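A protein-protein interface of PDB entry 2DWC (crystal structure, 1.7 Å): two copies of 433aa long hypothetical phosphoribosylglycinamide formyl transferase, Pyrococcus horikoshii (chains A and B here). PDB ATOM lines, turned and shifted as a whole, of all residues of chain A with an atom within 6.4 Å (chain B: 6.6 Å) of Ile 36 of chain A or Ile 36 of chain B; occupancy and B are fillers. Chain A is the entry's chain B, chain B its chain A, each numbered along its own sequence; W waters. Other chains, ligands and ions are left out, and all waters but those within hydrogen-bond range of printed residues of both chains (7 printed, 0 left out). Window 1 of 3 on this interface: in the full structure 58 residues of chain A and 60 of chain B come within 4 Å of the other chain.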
ATOM      1  N   GLY A  31     -22.751  -1.478  30.744  1.00  0.00           N
ATOM      2  CA  GLY A  31     -23.396  -0.456  31.558  1.00  0.00           C
ATOM      3  C   GLY A  31     -22.971   0.943  31.124  1.00  0.00           C
ATOM      4  O   GLY A  31     -23.739   1.913  31.198  1.00  0.00           O
ATOM      5  N   LYS A  32     -21.724   1.079  30.674  1.00  0.00           N
ATOM      6  CA  LYS A  32     -21.256   2.404  30.238  1.00  0.00           C
ATOM      7  C   LYS A  32     -22.101   2.918  29.066  1.00  0.00           C
ATOM      8  O   LYS A  32     -22.447   4.113  29.032  1.00  0.00           O
ATOM      9  CB  LYS A  32     -19.771   2.317  29.802  1.00  0.00           C
ATOM     10  CG  LYS A  32     -19.163   3.644  29.410  1.00  0.00           C
ATOM     11  CD  LYS A  32     -17.683   3.402  28.986  1.00  0.00           C
ATOM     12  CE  LYS A  32     -16.902   4.697  29.016  1.00  0.00           C
ATOM     13  NZ  LYS A  32     -15.494   4.456  28.507  1.00  0.00           N
ATOM     14  N   GLU A  33     -22.383   2.049  28.079  1.00  0.00           N
ATOM     15  CA  GLU A  33     -23.204   2.477  26.952  1.00  0.00           C
ATOM     16  C   GLU A  33     -24.677   2.731  27.347  1.00  0.00           C
ATOM     17  O   GLU A  33     -25.323   3.647  26.789  1.00  0.00           O
ATOM     18  CB  GLU A  33     -23.071   1.484  25.768  1.00  0.00           C
ATOM     19  CG  GLU A  33     -21.718   1.690  25.032  1.00  0.00           C
ATOM     20  CD  GLU A  33     -21.658   2.991  24.187  1.00  0.00           C
ATOM     21  OE1 GLU A  33     -20.515   3.391  23.809  1.00  0.00           O
ATOM     22  OE2 GLU A  33     -22.726   3.603  23.866  1.00  0.00           O
ATOM     23  N   ILE A  34     -25.207   2.002  28.335  1.00  0.00           N
ATOM     24  CA  ILE A  34     -26.572   2.314  28.798  1.00  0.00           C
ATOM     25  C   ILE A  34     -26.501   3.709  29.473  1.00  0.00           C
ATOM     26  O   ILE A  34     -27.371   4.561  29.302  1.00  0.00           O
ATOM     27  CB  ILE A  34     -27.057   1.291  29.849  1.00  0.00           C
ATOM     28  CG1 ILE A  34     -27.210  -0.089  29.182  1.00  0.00           C
ATOM     29  CG2 ILE A  34     -28.411   1.741  30.473  1.00  0.00           C
ATOM     30  CD1 ILE A  34     -27.432  -1.202  30.197  1.00  0.00           C
ATOM     31  N   ALA A  35     -25.427   3.965  30.220  1.00  0.00           N
ATOM     32  CA  ALA A  35     -25.309   5.259  30.872  1.00  0.00           C
ATOM     33  C   ALA A  35     -25.223   6.385  29.857  1.00  0.00           C
ATOM     34  O   ALA A  35     -25.750   7.486  30.081  1.00  0.00           O
ATOM     35  CB  ALA A  35     -24.049   5.273  31.811  1.00  0.00           C
ATOM     36  N   ILE A  36     -24.504   6.145  28.765  1.00  0.00           N
ATOM     37  CA  ILE A  36     -24.379   7.180  27.727  1.00  0.00           C
ATOM     38  C   ILE A  36     -25.742   7.475  27.089  1.00  0.00           C
ATOM     39  O   ILE A  36     -26.091   8.639  26.872  1.00  0.00           O
ATOM     40  CB  ILE A  36     -23.319   6.718  26.663  1.00  0.00           C
ATOM     41  CG1 ILE A  36     -21.926   6.937  27.241  1.00  0.00           C
ATOM     42  CG2 ILE A  36     -23.413   7.591  25.394  1.00  0.00           C
ATOM     43  CD1 ILE A  36     -20.832   6.309  26.403  1.00  0.00           C
ATOM     44  N   GLU A  37     -26.538   6.454  26.787  1.00  0.00           N
ATOM     45  CA  GLU A  37     -27.876   6.810  26.226  1.00  0.00           C
ATOM     46  C   GLU A  37     -28.739   7.515  27.264  1.00  0.00           C
ATOM     47  O   GLU A  37     -29.484   8.473  26.949  1.00  0.00           O
ATOM     48  CB  GLU A  37     -28.589   5.563  25.754  1.00  0.00           C
ATOM     49  CG  GLU A  37     -29.967   5.898  25.121  1.00  0.00           C
ATOM     50  CD  GLU A  37     -29.870   6.773  23.844  1.00  0.00           C
ATOM     51  OE1 GLU A  37     -28.804   6.805  23.141  1.00  0.00           O
ATOM     52  OE2 GLU A  37     -30.896   7.406  23.542  1.00  0.00           O
ATOM     53  N   ALA A  38     -28.618   7.082  28.513  1.00  0.00           N
ATOM     54  CA  ALA A  38     -29.404   7.768  29.575  1.00  0.00           C
ATOM     55  C   ALA A  38     -28.997   9.243  29.635  1.00  0.00           C
ATOM     56  O   ALA A  38     -29.833  10.140  29.676  1.00  0.00           O
ATOM     57  CB  ALA A  38     -29.147   7.090  30.929  1.00  0.00           C
ATOM     58  N   GLN A  39     -27.688   9.514  29.654  1.00  0.00           N
ATOM     59  CA  GLN A  39     -27.245  10.923  29.647  1.00  0.00           C
ATOM     60  C   GLN A  39     -27.770  11.656  28.442  1.00  0.00           C
ATOM     61  O   GLN A  39     -28.124  12.822  28.528  1.00  0.00           O
ATOM     62  CB  GLN A  39     -25.725  11.039  29.632  1.00  0.00           C
ATOM     63  CG  GLN A  39     -25.137  10.581  30.984  1.00  0.00           C
ATOM     64  CD  GLN A  39     -25.053  11.707  32.009  1.00  0.00           C
ATOM     65  OE1 GLN A  39     -25.729  12.723  31.912  1.00  0.00           O
ATOM     66  NE2 GLN A  39     -24.196  11.523  33.006  1.00  0.00           N
ATOM     67  N   ARG A  40     -27.798  10.995  27.300  1.00  0.00           N
ATOM     68  CA  ARG A  40     -28.319  11.617  26.101  1.00  0.00           C
ATOM     69  C   ARG A  40     -29.820  11.946  26.142  1.00  0.00           C
ATOM     70  O   ARG A  40     -30.277  12.770  25.344  1.00  0.00           O
ATOM     71  CB  ARG A  40     -27.996  10.749  24.890  1.00  0.00           C
ATOM     72  CG  ARG A  40     -26.572  10.984  24.382  1.00  0.00           C
ATOM     73  CD  ARG A  40     -26.238   9.981  23.300  1.00  0.00           C
ATOM     74  NE  ARG A  40     -25.033  10.416  22.549  1.00  0.00           N
ATOM     75  CZ  ARG A  40     -24.437   9.639  21.656  1.00  0.00           C
ATOM     76  NH1 ARG A  40     -24.894   8.394  21.425  1.00  0.00           N
ATOM     77  NH2 ARG A  40     -23.454  10.137  20.925  1.00  0.00           N
ATOM     78  N   LEU A  41     -30.543  11.362  27.105  1.00  0.00           N
ATOM     79  CA  LEU A  41     -31.975  11.618  27.289  1.00  0.00           C
ATOM     80  C   LEU A  41     -32.198  12.432  28.586  1.00  0.00           C
ATOM     81  O   LEU A  41     -33.331  12.618  29.021  1.00  0.00           O
ATOM     82  CB  LEU A  41     -32.726  10.295  27.380  1.00  0.00           C
ATOM     83  CG  LEU A  41     -32.785   9.470  26.104  1.00  0.00           C
ATOM     84  CD1 LEU A  41     -33.498   8.157  26.352  1.00  0.00           C
ATOM     85  CD2 LEU A  41     -33.556  10.272  25.060  1.00  0.00           C
ATOM     86  N   VAL A  45     -28.151   8.894  36.247  1.00  0.00           N
ATOM     87  CA  VAL A  45     -27.541   7.557  36.337  1.00  0.00           C
ATOM     88  C   VAL A  45     -26.706   7.357  37.590  1.00  0.00           C
ATOM     89  O   VAL A  45     -25.832   8.176  37.878  1.00  0.00           O
ATOM     90  CB  VAL A  45     -26.546   7.322  35.154  1.00  0.00           C
ATOM     91  CG1 VAL A  45     -25.967   5.892  35.202  1.00  0.00           C
ATOM     92  CG2 VAL A  45     -27.287   7.513  33.833  1.00  0.00           C
ATOM     93  N   VAL A  59     -19.008   7.849  33.416  1.00  0.00           N
ATOM     94  CA  VAL A  59     -20.034   8.585  32.660  1.00  0.00           C
ATOM     95  C   VAL A  59     -21.271   8.917  33.521  1.00  0.00           C
ATOM     96  O   VAL A  59     -21.970   9.876  33.253  1.00  0.00           O
ATOM     97  CB  VAL A  59     -20.484   7.753  31.435  1.00  0.00           C
ATOM     98  CG1 VAL A  59     -21.803   8.307  30.851  1.00  0.00           C
ATOM     99  CG2 VAL A  59     -19.358   7.847  30.344  1.00  0.00           C
ATOM    100  N   LEU A 318     -32.581   0.535  27.567  1.00  0.00           N
ATOM    101  CA  LEU A 318     -32.949   1.687  28.390  1.00  0.00           C
ATOM    102  C   LEU A 318     -34.378   2.169  28.087  1.00  0.00           C
ATOM    103  O   LEU A 318     -35.176   2.447  28.992  1.00  0.00           O
ATOM    104  CB  LEU A 318     -31.961   2.839  28.154  1.00  0.00           C
ATOM    105  CG  LEU A 318     -32.307   4.110  28.940  1.00  0.00           C
ATOM    106  CD1 LEU A 318     -32.144   3.847  30.444  1.00  0.00           C
ATOM    107  CD2 LEU A 318     -31.385   5.252  28.495  1.00  0.00           C
ATOM    108  N   GLY B  31     -20.407  20.625  23.877  1.00  0.00           N
ATOM    109  CA  GLY B  31     -19.370  20.092  24.762  1.00  0.00           C
ATOM    110  C   GLY B  31     -19.772  18.704  25.304  1.00  0.00           C
ATOM    111  O   GLY B  31     -18.926  17.842  25.516  1.00  0.00           O
ATOM    112  N   LYS B  32     -21.069  18.497  25.542  1.00  0.00           N
ATOM    113  CA  LYS B  32     -21.549  17.202  26.056  1.00  0.00           C
ATOM    114  C   LYS B  32     -21.233  16.078  25.083  1.00  0.00           C
ATOM    115  O   LYS B  32     -20.790  14.974  25.510  1.00  0.00           O
ATOM    116  CB  LYS B  32     -23.084  17.281  26.267  1.00  0.00           C
ATOM    117  CG  LYS B  32     -23.631  16.057  27.002  1.00  0.00           C
ATOM    118  CD  LYS B  32     -25.141  16.183  27.108  1.00  0.00           C
ATOM    119  CE  LYS B  32     -25.696  15.096  28.068  1.00  0.00           C
ATOM    120  NZ  LYS B  32     -27.195  15.347  28.218  1.00  0.00           N
ATOM    121  N   GLU B  33     -21.443  16.327  23.788  1.00  0.00           N
ATOM    122  CA  GLU B  33     -21.154  15.286  22.798  1.00  0.00           C
ATOM    123  C   GLU B  33     -19.639  15.084  22.615  1.00  0.00           C
ATOM    124  O   GLU B  33     -19.196  13.953  22.363  1.00  0.00           O
ATOM    125  CB  GLU B  33     -21.865  15.557  21.461  1.00  0.00           C
ATOM    126  CG  GLU B  33     -23.379  15.197  21.563  1.00  0.00           C
ATOM    127  CD  GLU B  33     -23.639  13.670  21.583  1.00  0.00           C
ATOM    128  OE1 GLU B  33     -24.757  13.265  21.951  1.00  0.00           O
ATOM    129  OE2 GLU B  33     -22.760  12.834  21.215  1.00  0.00           O
ATOM    130  N   ILE B  34     -18.864  16.154  22.751  1.00  0.00           N
ATOM    131  CA  ILE B  34     -17.403  16.005  22.720  1.00  0.00           C
ATOM    132  C   ILE B  34     -17.021  15.144  23.929  1.00  0.00           C
ATOM    133  O   ILE B  34     -16.197  14.216  23.828  1.00  0.00           O
ATOM    134  CB  ILE B  34     -16.668  17.367  22.819  1.00  0.00           C
ATOM    135  CG1 ILE B  34     -16.905  18.147  21.511  1.00  0.00           C
ATOM    136  CG2 ILE B  34     -15.136  17.147  23.023  1.00  0.00           C
ATOM    137  CD1 ILE B  34     -16.270  19.527  21.509  1.00  0.00           C
ATOM    138  N   ALA B  35     -17.636  15.418  25.083  1.00  0.00           N
ATOM    139  CA  ALA B  35     -17.299  14.623  26.281  1.00  0.00           C
ATOM    140  C   ALA B  35     -17.678  13.155  26.138  1.00  0.00           C
ATOM    141  O   ALA B  35     -16.976  12.270  26.635  1.00  0.00           O
ATOM    142  CB  ALA B  35     -17.997  15.255  27.519  1.00  0.00           C
ATOM    143  N   ILE B  36     -18.808  12.865  25.504  1.00  0.00           N
ATOM    144  CA  ILE B  36     -19.201  11.472  25.308  1.00  0.00           C
ATOM    145  C   ILE B  36     -18.183  10.741  24.400  1.00  0.00           C
ATOM    146  O   ILE B  36     -17.797   9.605  24.688  1.00  0.00           O
ATOM    147  CB  ILE B  36     -20.631  11.429  24.697  1.00  0.00           C
ATOM    148  CG1 ILE B  36     -21.623  11.860  25.789  1.00  0.00           C
ATOM    149  CG2 ILE B  36     -20.947  10.025  24.124  1.00  0.00           C
ATOM    150  CD1 ILE B  36     -23.058  12.080  25.254  1.00  0.00           C
ATOM    151  N   GLU B  37     -17.748  11.382  23.307  1.00  0.00           N
ATOM    152  CA  GLU B  37     -16.755  10.702  22.466  1.00  0.00           C
ATOM    153  C   GLU B  37     -15.461  10.527  23.236  1.00  0.00           C
ATOM    154  O   GLU B  37     -14.811   9.480  23.129  1.00  0.00           O
ATOM    155  CB  GLU B  37     -16.478  11.479  21.184  1.00  0.00           C
ATOM    156  CG  GLU B  37     -15.515  10.690  20.231  1.00  0.00           C
ATOM    157  CD  GLU B  37     -16.011   9.283  19.817  1.00  0.00           C
ATOM    158  OE1 GLU B  37     -17.258   9.030  19.674  1.00  0.00           O
ATOM    159  OE2 GLU B  37     -15.125   8.433  19.603  1.00  0.00           O
ATOM    160  N   ALA B  38     -15.077  11.540  24.025  1.00  0.00           N
ATOM    161  CA  ALA B  38     -13.861  11.379  24.845  1.00  0.00           C
ATOM    162  C   ALA B  38     -14.033  10.176  25.805  1.00  0.00           C
ATOM    163  O   ALA B  38     -13.141   9.310  25.915  1.00  0.00           O
ATOM    164  CB  ALA B  38     -13.597  12.680  25.651  1.00  0.00           C
ATOM    165  N   GLN B  39     -15.165  10.102  26.516  1.00  0.00           N
ATOM    166  CA  GLN B  39     -15.399   8.960  27.415  1.00  0.00           C
ATOM    167  C   GLN B  39     -15.339   7.645  26.636  1.00  0.00           C
ATOM    168  O   GLN B  39     -14.840   6.639  27.118  1.00  0.00           O
ATOM    169  CB  GLN B  39     -16.775   9.087  28.089  1.00  0.00           C
ATOM    170  CG  GLN B  39     -16.774  10.230  29.096  1.00  0.00           C
ATOM    171  CD  GLN B  39     -16.286   9.774  30.449  1.00  0.00           C
ATOM    172  OE1 GLN B  39     -15.651   8.711  30.591  1.00  0.00           O
ATOM    173  NE2 GLN B  39     -16.586  10.578  31.479  1.00  0.00           N
ATOM    174  N   ARG B  40     -15.811   7.650  25.398  1.00  0.00           N
ATOM    175  CA  ARG B  40     -15.785   6.414  24.640  1.00  0.00           C
ATOM    176  C   ARG B  40     -14.377   5.984  24.220  1.00  0.00           C
ATOM    177  O   ARG B  40     -14.166   4.842  23.806  1.00  0.00           O
ATOM    178  CB  ARG B  40     -16.695   6.554  23.408  1.00  0.00           C
ATOM    179  CG  ARG B  40     -18.172   6.275  23.785  1.00  0.00           C
ATOM    180  CD  ARG B  40     -19.091   6.721  22.663  1.00  0.00           C
ATOM    181  NE  ARG B  40     -20.417   6.075  22.720  1.00  0.00           N
ATOM    182  CZ  ARG B  40     -21.400   6.381  21.882  1.00  0.00           C
ATOM    183  NH1 ARG B  40     -21.225   7.327  20.943  1.00  0.00           N
ATOM    184  NH2 ARG B  40     -22.528   5.682  21.923  1.00  0.00           N
ATOM    185  N   LEU B  41     -13.421   6.898  24.337  1.00  0.00           N
ATOM    186  CA  LEU B  41     -12.037   6.588  24.008  1.00  0.00           C
ATOM    187  C   LEU B  41     -11.201   6.507  25.290  1.00  0.00           C
ATOM    188  O   LEU B  41      -9.970   6.440  25.218  1.00  0.00           O
ATOM    189  CB  LEU B  41     -11.441   7.650  23.073  1.00  0.00           C
ATOM    190  CG  LEU B  41     -11.987   7.626  21.633  1.00  0.00           C
ATOM    191  CD1 LEU B  41     -11.419   8.837  20.856  1.00  0.00           C
ATOM    192  CD2 LEU B  41     -11.603   6.304  20.921  1.00  0.00           C
ATOM    193  N   VAL B  45     -12.032  13.955  31.005  1.00  0.00           N
ATOM    194  CA  VAL B  45     -12.740  15.178  30.610  1.00  0.00           C
ATOM    195  C   VAL B  45     -12.988  16.074  31.808  1.00  0.00           C
ATOM    196  O   VAL B  45     -13.533  15.638  32.816  1.00  0.00           O
ATOM    197  CB  VAL B  45     -14.157  14.831  30.039  1.00  0.00           C
ATOM    198  CG1 VAL B  45     -14.886  16.130  29.573  1.00  0.00           C
ATOM    199  CG2 VAL B  45     -14.014  13.889  28.847  1.00  0.00           C
ATOM    200  N   VAL B  59     -21.572  14.528  32.098  1.00  0.00           N
ATOM    201  CA  VAL B  59     -20.857  13.400  31.489  1.00  0.00           C
ATOM    202  C   VAL B  59     -19.359  13.398  31.817  1.00  0.00           C
ATOM    203  O   VAL B  59     -18.722  12.346  31.817  1.00  0.00           O
ATOM    204  CB  VAL B  59     -21.064  13.438  29.958  1.00  0.00           C
ATOM    205  CG1 VAL B  59     -20.092  12.530  29.265  1.00  0.00           C
ATOM    206  CG2 VAL B  59     -22.554  13.031  29.660  1.00  0.00           C
ATOM    207  N   LEU B 318     -12.710  16.089  18.355  1.00  0.00           N
ATOM    208  CA  LEU B 318     -11.911  15.465  19.400  1.00  0.00           C
ATOM    209  C   LEU B 318     -10.674  14.753  18.804  1.00  0.00           C
ATOM    210  O   LEU B 318      -9.531  14.925  19.266  1.00  0.00           O
ATOM    211  CB  LEU B 318     -12.776  14.494  20.203  1.00  0.00           C
ATOM    212  CG  LEU B 318     -11.937  13.772  21.279  1.00  0.00           C
ATOM    213  CD1 LEU B 318     -11.465  14.728  22.360  1.00  0.00           C
ATOM    214  CD2 LEU B 318     -12.811  12.652  21.833  1.00  0.00           C
HETATM  215  O   HOH W   1     -15.986   3.093  25.835  1.00  0.00           O
HETATM  216  O   HOH W   2     -26.403  11.420  19.783  1.00  0.00           O
HETATM  217  O   HOH W   3     -28.122  15.072  25.317  1.00  0.00           O
HETATM  218  O   HOH W   4     -19.837  11.766  34.944  1.00  0.00           O
HETATM  219  O   HOH W   5     -27.761  14.568  31.078  1.00  0.00           O
HETATM  220  O   HOH W   6     -13.898   6.534  30.089  1.00  0.00           O
HETATM  221  O   HOH W   7     -20.319   3.583  20.623  1.00  0.00           O
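NH2 of Arg 40 of chain A lies within salt-bridge range of OE2 of Glu 33 of chain B, 2.8 Å away.
The side-chain amino group (NZ) of Lys 32 of chain B is in hydrogen-bond range of the backbone carbonyl oxygen (O) of Gln 39 of chain A, 2.7 Å away.
O of Gln 39 of chain B lies within hydrogen-bond range of NZ of Lys 32 of chain A.
NH2 of Arg 40 of chain B lies within salt-bridge range of OE2 of Glu 33 of chain A, at 2.9 Å.
NE2 of Gln 39 of chain B is in hydrogen-bond range of O of Val 59 of chain B.
NE2 of Gln 39 of chain A lies within hydrogen-bond range of O of Val 59 of chain A (2.8 Å).
Among the printed residues, pairs that only touch across the chains: Arg 40 of chain A with Arg 40 of chain B (3.6 Å), Val 59 of chain A with Gln 39 of chain B (3.6 Å), Gln 39 of chain A with Val 59 of chain B (3.7 Å), Ile 36 of chain A with Ile 36 of chain B (3.7 Å), Ile 36 of chain A with Arg 40 of chain B (3.7 Å) and Arg 40 of chain A with Ile 36 of chain B (3.7 Å).
Ile 36 of chain A touches two residues of chain B.
Of the printed residues of chain B, Gln 39 of chain A touches Lys 32 (2.7 Å) and Val 59 (3.7 Å).
Leu 41 of chain A touches none of the printed residues of chain B.
Ile 34 of chain B touches none of the printed residues of chain A.
Ile 36 of chain B touches just these residues of chain A: Ile 36 (3.7 Å) and Arg 40 (3.7 Å).
Printed residues of chain A within 4 Å of Gln 39 of chain B: Lys 32 (2.7 Å) and Val 59 (3.6 Å).
Of the printed residues of chain A, Arg 40 of chain B touches Glu 33, Ile 36 and Arg 40.
Printed residues of chain A within 4 Å of Val 59 of chain B: Gln 39 (3.7 Å).
The nearest printed residue of chain A that does not touch Lys 32 of chain B is Arg 40 of chain A (4.4 Å).
Hydrophobic or aromatic side chains of chain B within 4 Å of the printed part of chain A: Ile 36 and Val 59.
Among the printed residues, 10 pairs touch across the chains.
Among the printed residues, Asp or Glu carboxylates within 4 Å of a Lys or Arg side-chain nitrogen of the other chain: Glu 33 of chain A with Arg 40 of chain B and Arg 40 of chain A with Glu 33 of chain B.
Glu 33 of chain A touches Arg 40 of chain B, and with the chains exchanged Arg 40 of chain A touches Glu 33 of chain B.
Ile 36 of chain B touches its own counterpart, Ile 36 of chain A.
Ile 36 of chain A touches Arg 40 of chain B, and with the chains exchanged Arg 40 of chain A touches Ile 36 of chain B.
Gln 39 of chain A touches Val 59 of chain B, and with the chains exchanged Val 59 of chain A touches Gln 39 of chain B.
Of the 10 pairs that touch across the chains among the printed residues, 10 have their exchanged pair printed and touching as well.
Water W5 bridges OE1 of Gln 39 of chain A (2.9 Å) and NZ of Lys 32 of chain B (3.0 Å).
Water W1 lies within hydrogen-bond range of the side-chain amino group of Lys 32 of chain A (3.0 Å) and the backbone carbonyl oxygen of Arg 40 of chain B (3.2 Å).
Water W3 lies within hydrogen-bond range of NZ of Lys 32 of chain B (3.1 Å) and O of Arg 40 of chain A (3.2 Å).
Water W7 bridges the side-chain carboxylate of Glu 33 of chain A and the guanidinium group of Arg 40 of chain B.
Water W2 lies within hydrogen-bond range of the guanidinium group of Arg 40 of chain A and the side-chain carboxylate of Glu 33 of chain B.
Water W4 lies within hydrogen-bond range of O of Val 59 of chain A (3.3 Å) and O of Val 59 of chain B (3.4 Å).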
